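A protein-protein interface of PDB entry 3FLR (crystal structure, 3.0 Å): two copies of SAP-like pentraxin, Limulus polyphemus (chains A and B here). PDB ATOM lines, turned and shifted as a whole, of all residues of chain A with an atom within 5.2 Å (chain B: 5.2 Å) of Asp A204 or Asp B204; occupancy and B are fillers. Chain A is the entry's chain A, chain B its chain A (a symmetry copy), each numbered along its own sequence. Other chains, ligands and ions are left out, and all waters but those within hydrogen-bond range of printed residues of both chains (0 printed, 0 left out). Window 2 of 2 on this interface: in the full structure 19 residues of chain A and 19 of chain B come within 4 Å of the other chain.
Ala A203 touches Gly B206, and with the chains exchanged Gly A206 touches Ala B203. Asp B204 touches its own counterpart, Asp A204. Asp A204 touches Asp B205, and with the chains exchanged Asp A205 touches Asp B204. Asp A204 touches Gly B206, and with the chains exchanged Gly A206 touches Asp B204. Of the 13 pairs that touch across the chains among the printed residues, 13 have their exchanged pair printed and touching as well.
CG1 of Val A202 touches CA of Gly B206, at 3.6 Å. Val A202 touches Val B207 (CA to O, 3.7 Å). Asp A204 touches Gly B206 (OD2 to N, 3.8 Å). Gly A206 touches Val B202. Gly A206 touches Asp B204. Val A207 touches Val B202 (O to CA, 3.7 Å).
The backbone carbonyl oxygen (O) of Ala A203 lies within hydrogen-bond range of the backbone NH (N) of Gly B206 (3.1 Å). The backbone NH (N) of Ala A203 is in hydrogen-bond range of the backbone carbonyl oxygen (O) of Val B207. The side-chain carboxylate (OD1) of Asp B204 sits close to the side-chain carboxylate (OD1) of Asp A204 (2.4 Å). OD1 of Asp A204 sits at hydrogen-bond distance from N of Asp B205 (3.2 Å). The side-chain carboxylate (OD1) of Asp B204 is in hydrogen-bond range of the backbone NH (N) of Asp A205. N of Gly A206 lies within hydrogen-bond range of O of Ala B203. The backbone carbonyl oxygen (O) of Val A207 sits at hydrogen-bond distance from the backbone NH (N) of Ala B203 (3.1 Å).
Asp A204 touches just these residues of chain B: Asp B204, Asp B205 and Gly B206. Of the printed residues of chain B, Asp A205 touches Asp B204 (3.2 Å). Of the printed residues of chain A, Val B202 touches Gly A206 (3.6 Å) and Val A207 (3.7 Å). Asp B204 touches just these residues of chain A: Asp A204, Asp A205 and Gly A206. Of the printed residues of chain A, Asp B205 touches Asp A204 (3.2 Å). Of the printed residues of chain A, Gly B206 touches Val A202 (3.6 Å), Ala A203 (3.1 Å) and Asp A204 (3.8 Å). The nearest residue of chain B that does not touch Asp A204 is Ala B203 (4.2 Å). The nearest printed residue of chain A that does not touch Ala B203 is Asp A205 (4.2 Å).
Of the 9 printed residues of chain A, 6 touch a printed residue of chain B. Hydrophobic or aromatic side chains of chain A that line the printed part of chain B: Val A202. Of the 9 printed residues of chain B, 6 touch a printed residue of chain A. Among the printed residues, no Asp or Glu carboxylate lies within 4 Å of a Lys or Arg side-chain nitrogen of the other chain.
The side-chain carboxylate of Asp A205 is in hydrogen-bond range of the backbone NH of Phe A19. O of Asp A204 sits at hydrogen-bond distance from N of His A21 (3.4 Å). OD1 of Asp A204 lies close to OD1 of Asp A205 (2.6 Å). The backbone NH (N) of Phe B19 lies within hydrogen-bond range of the side-chain carboxylate (OD2) of Asp B205 (2.8 Å). The backbone NH of His B21 lies within hydrogen-bond range of the backbone carbonyl oxygen of Asp B204. OD1 of Asp B205 sits close to OD1 of Asp B204 (2.6 Å).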
ATOM      1  N   PHE A  19     -13.352  -8.263  -9.876  1.00  0.00           N
ATOM      2  CA  PHE A  19     -12.895  -9.390 -10.679  1.00  0.00           C
ATOM      3  C   PHE A  19     -11.687  -9.052 -11.544  1.00  0.00           C
ATOM      4  O   PHE A  19     -11.799  -8.956 -12.766  1.00  0.00           O
ATOM      5  CB  PHE A  19     -14.022  -9.880 -11.594  1.00  0.00           C
ATOM      6  CG  PHE A  19     -15.198 -10.430 -10.863  1.00  0.00           C
ATOM      7  CD1 PHE A  19     -16.168  -9.585 -10.354  1.00  0.00           C
ATOM      8  CD2 PHE A  19     -15.315 -11.799 -10.653  1.00  0.00           C
ATOM      9  CE1 PHE A  19     -17.236 -10.090  -9.643  1.00  0.00           C
ATOM     10  CE2 PHE A  19     -16.374 -12.319  -9.946  1.00  0.00           C
ATOM     11  CZ  PHE A  19     -17.343 -11.464  -9.436  1.00  0.00           C
ATOM     12  N   PRO A  20     -10.508  -8.894 -10.931  1.00  0.00           N
ATOM     13  CA  PRO A  20      -9.325  -8.566 -11.735  1.00  0.00           C
ATOM     14  C   PRO A  20      -9.186  -9.501 -12.936  1.00  0.00           C
ATOM     15  O   PRO A  20      -9.230 -10.724 -12.789  1.00  0.00           O
ATOM     16  CB  PRO A  20      -8.177  -8.699 -10.732  1.00  0.00           C
ATOM     17  CG  PRO A  20      -8.673  -9.733  -9.792  1.00  0.00           C
ATOM     18  CD  PRO A  20     -10.114  -9.334  -9.582  1.00  0.00           C
ATOM     19  N   HIS A  21      -9.027  -8.915 -14.121  1.00  0.00           N
ATOM     20  CA  HIS A  21      -8.910  -9.697 -15.345  1.00  0.00           C
ATOM     21  C   HIS A  21      -8.413  -8.876 -16.549  1.00  0.00           C
ATOM     22  O   HIS A  21      -8.234  -7.657 -16.474  1.00  0.00           O
ATOM     23  CB  HIS A  21     -10.273 -10.264 -15.703  1.00  0.00           C
ATOM     24  CG  HIS A  21     -11.227  -9.220 -16.190  1.00  0.00           C
ATOM     25  ND1 HIS A  21     -11.813  -8.301 -15.348  1.00  0.00           N
ATOM     26  CD2 HIS A  21     -11.613  -8.882 -17.443  1.00  0.00           C
ATOM     27  CE1 HIS A  21     -12.517  -7.441 -16.061  1.00  0.00           C
ATOM     28  NE2 HIS A  21     -12.412  -7.771 -17.335  1.00  0.00           N
ATOM     29  N   VAL A 202      -7.555  -5.112 -22.587  1.00  0.00           N
ATOM     30  CA  VAL A 202      -8.130  -4.201 -21.588  1.00  0.00           C
ATOM     31  C   VAL A 202      -7.926  -4.728 -20.170  1.00  0.00           C
ATOM     32  O   VAL A 202      -7.989  -5.938 -19.940  1.00  0.00           O
ATOM     33  CB  VAL A 202      -9.657  -4.013 -21.787  1.00  0.00           C
ATOM     34  CG1 VAL A 202     -10.133  -2.807 -21.004  1.00  0.00           C
ATOM     35  CG2 VAL A 202      -9.983  -3.865 -23.260  1.00  0.00           C
ATOM     36  N   ALA A 203      -7.698  -3.827 -19.217  1.00  0.00           N
ATOM     37  CA  ALA A 203      -7.497  -4.235 -17.828  1.00  0.00           C
ATOM     38  C   ALA A 203      -8.490  -3.568 -16.888  1.00  0.00           C
ATOM     39  O   ALA A 203      -8.888  -2.425 -17.107  1.00  0.00           O
ATOM     40  CB  ALA A 203      -6.077  -3.912 -17.391  1.00  0.00           C
ATOM     41  N   ASP A 204      -8.889  -4.283 -15.839  1.00  0.00           N
ATOM     42  CA  ASP A 204      -9.828  -3.736 -14.859  1.00  0.00           C
ATOM     43  C   ASP A 204      -9.689  -4.465 -13.534  1.00  0.00           C
ATOM     44  O   ASP A 204      -9.120  -5.551 -13.454  1.00  0.00           O
ATOM     45  CB  ASP A 204     -11.277  -3.898 -15.334  1.00  0.00           C
ATOM     46  CG  ASP A 204     -12.260  -2.929 -14.643  1.00  0.00           C
ATOM     47  OD1 ASP A 204     -12.143  -2.581 -13.436  1.00  0.00           O
ATOM     48  OD2 ASP A 204     -13.201  -2.517 -15.338  1.00  0.00           O
ATOM     49  N   ASP A 205     -10.228  -3.844 -12.498  1.00  0.00           N
ATOM     50  CA  ASP A 205     -10.258  -4.398 -11.152  1.00  0.00           C
ATOM     51  C   ASP A 205      -8.962  -4.756 -10.453  1.00  0.00           C
ATOM     52  O   ASP A 205      -8.837  -5.816  -9.841  1.00  0.00           O
ATOM     53  CB  ASP A 205     -11.230  -5.575 -11.109  1.00  0.00           C
ATOM     54  CG  ASP A 205     -12.660  -5.127 -11.294  1.00  0.00           C
ATOM     55  OD1 ASP A 205     -12.906  -3.887 -11.284  1.00  0.00           O
ATOM     56  OD2 ASP A 205     -13.538  -5.999 -11.447  1.00  0.00           O
ATOM     57  N   GLY A 206      -7.996  -3.852 -10.551  1.00  0.00           N
ATOM     58  CA  GLY A 206      -6.735  -4.023  -9.854  1.00  0.00           C
ATOM     59  C   GLY A 206      -5.633  -4.962 -10.286  1.00  0.00           C
ATOM     60  O   GLY A 206      -4.881  -5.405  -9.419  1.00  0.00           O
ATOM     61  N   VAL A 207      -5.516  -5.281 -11.574  1.00  0.00           N
ATOM     62  CA  VAL A 207      -4.419  -6.147 -12.002  1.00  0.00           C
ATOM     63  C   VAL A 207      -3.154  -5.317 -11.823  1.00  0.00           C
ATOM     64  O   VAL A 207      -3.162  -4.108 -12.066  1.00  0.00           O
ATOM     65  CB  VAL A 207      -4.514  -6.550 -13.492  1.00  0.00           C
ATOM     66  CG1 VAL A 207      -5.748  -7.390 -13.730  1.00  0.00           C
ATOM     67  CG2 VAL A 207      -4.523  -5.312 -14.372  1.00  0.00           C
ATOM     68  N   PHE B  19     -13.584   5.328 -13.796  1.00  0.00           N
ATOM     69  CA  PHE B  19     -12.456   6.250 -13.799  1.00  0.00           C
ATOM     70  C   PHE B  19     -11.148   5.586 -14.211  1.00  0.00           C
ATOM     71  O   PHE B  19     -10.257   5.390 -13.384  1.00  0.00           O
ATOM     72  CB  PHE B  19     -12.269   6.862 -12.406  1.00  0.00           C
ATOM     73  CG  PHE B  19     -13.410   7.711 -11.961  1.00  0.00           C
ATOM     74  CD1 PHE B  19     -14.539   7.137 -11.405  1.00  0.00           C
ATOM     75  CD2 PHE B  19     -13.366   9.090 -12.134  1.00  0.00           C
ATOM     76  CE1 PHE B  19     -15.611   7.919 -11.030  1.00  0.00           C
ATOM     77  CE2 PHE B  19     -14.427   9.884 -11.765  1.00  0.00           C
ATOM     78  CZ  PHE B  19     -15.557   9.301 -11.209  1.00  0.00           C
ATOM     79  N   PRO B  20     -10.997   5.257 -15.499  1.00  0.00           N
ATOM     80  CA  PRO B  20      -9.749   4.615 -15.928  1.00  0.00           C
ATOM     81  C   PRO B  20      -8.524   5.373 -15.421  1.00  0.00           C
ATOM     82  O   PRO B  20      -8.418   6.588 -15.599  1.00  0.00           O
ATOM     83  CB  PRO B  20      -9.868   4.614 -17.454  1.00  0.00           C
ATOM     84  CG  PRO B  20     -10.689   5.819 -17.725  1.00  0.00           C
ATOM     85  CD  PRO B  20     -11.758   5.744 -16.662  1.00  0.00           C
ATOM     86  N   HIS B  21      -7.608   4.648 -14.781  1.00  0.00           N
ATOM     87  CA  HIS B  21      -6.407   5.259 -14.226  1.00  0.00           C
ATOM     88  C   HIS B  21      -5.332   4.235 -13.820  1.00  0.00           C
ATOM     89  O   HIS B  21      -5.537   3.020 -13.882  1.00  0.00           O
ATOM     90  CB  HIS B  21      -6.783   6.051 -12.985  1.00  0.00           C
ATOM     91  CG  HIS B  21      -7.151   5.178 -11.828  1.00  0.00           C
ATOM     92  ND1 HIS B  21      -8.341   4.489 -11.767  1.00  0.00           N
ATOM     93  CD2 HIS B  21      -6.441   4.799 -10.739  1.00  0.00           C
ATOM     94  CE1 HIS B  21      -8.349   3.721 -10.693  1.00  0.00           C
ATOM     95  NE2 HIS B  21      -7.207   3.890 -10.052  1.00  0.00           N
ATOM     96  N   VAL B 202      -0.797  -0.227 -10.519  1.00  0.00           N
ATOM     97  CA  VAL B 202      -2.105  -0.894 -10.562  1.00  0.00           C
ATOM     98  C   VAL B 202      -3.012  -0.276 -11.624  1.00  0.00           C
ATOM     99  O   VAL B 202      -2.986   0.939 -11.835  1.00  0.00           O
ATOM    100  CB  VAL B 202      -2.855  -0.787  -9.207  1.00  0.00           C
ATOM    101  CG1 VAL B 202      -3.995  -1.784  -9.171  1.00  0.00           C
ATOM    102  CG2 VAL B 202      -1.897  -1.017  -8.056  1.00  0.00           C
ATOM    103  N   ALA B 203      -3.824  -1.102 -12.280  1.00  0.00           N
ATOM    104  CA  ALA B 203      -4.733  -0.602 -13.309  1.00  0.00           C
ATOM    105  C   ALA B 203      -6.183  -0.953 -13.010  1.00  0.00           C
ATOM    106  O   ALA B 203      -6.468  -2.008 -12.445  1.00  0.00           O
ATOM    107  CB  ALA B 203      -4.339  -1.160 -14.667  1.00  0.00           C
ATOM    108  N   ASP B 204      -7.101  -0.067 -13.390  1.00  0.00           N
ATOM    109  CA  ASP B 204      -8.527  -0.309 -13.170  1.00  0.00           C
ATOM    110  C   ASP B 204      -9.356   0.510 -14.144  1.00  0.00           C
ATOM    111  O   ASP B 204      -8.875   1.460 -14.758  1.00  0.00           O
ATOM    112  CB  ASP B 204      -8.941   0.094 -11.749  1.00  0.00           C
ATOM    113  CG  ASP B 204     -10.248  -0.579 -11.278  1.00  0.00           C
ATOM    114  OD1 ASP B 204     -11.214  -0.816 -12.054  1.00  0.00           O
ATOM    115  OD2 ASP B 204     -10.313  -0.861 -10.072  1.00  0.00           O
ATOM    116  N   ASP B 205     -10.614   0.121 -14.268  1.00  0.00           N
ATOM    117  CA  ASP B 205     -11.591   0.805 -15.103  1.00  0.00           C
ATOM    118  C   ASP B 205     -11.337   0.962 -16.589  1.00  0.00           C
ATOM    119  O   ASP B 205     -11.538   2.032 -17.162  1.00  0.00           O
ATOM    120  CB  ASP B 205     -11.939   2.153 -14.476  1.00  0.00           C
ATOM    121  CG  ASP B 205     -12.697   1.987 -13.180  1.00  0.00           C
ATOM    122  OD1 ASP B 205     -13.097   0.832 -12.863  1.00  0.00           O
ATOM    123  OD2 ASP B 205     -12.899   2.999 -12.480  1.00  0.00           O
ATOM    124  N   GLY B 206     -10.892  -0.124 -17.207  1.00  0.00           N
ATOM    125  CA  GLY B 206     -10.695  -0.141 -18.644  1.00  0.00           C
ATOM    126  C   GLY B 206      -9.533   0.505 -19.361  1.00  0.00           C
ATOM    127  O   GLY B 206      -9.705   0.873 -20.523  1.00  0.00           O
ATOM    128  N   VAL B 207      -8.375   0.659 -18.721  1.00  0.00           N
ATOM    129  CA  VAL B 207      -7.234   1.236 -19.428  1.00  0.00           C
ATOM    130  C   VAL B 207      -6.825   0.189 -20.458  1.00  0.00           C
ATOM    131  O   VAL B 207      -6.881  -1.012 -20.182  1.00  0.00           O
ATOM    132  CB  VAL B 207      -6.019   1.494 -18.507  1.00  0.00           C
ATOM    133  CG1 VAL B 207      -6.362   2.538 -17.469  1.00  0.00           C
ATOM    134  CG2 VAL B 207      -5.574   0.199 -17.848  1.00  0.00           C
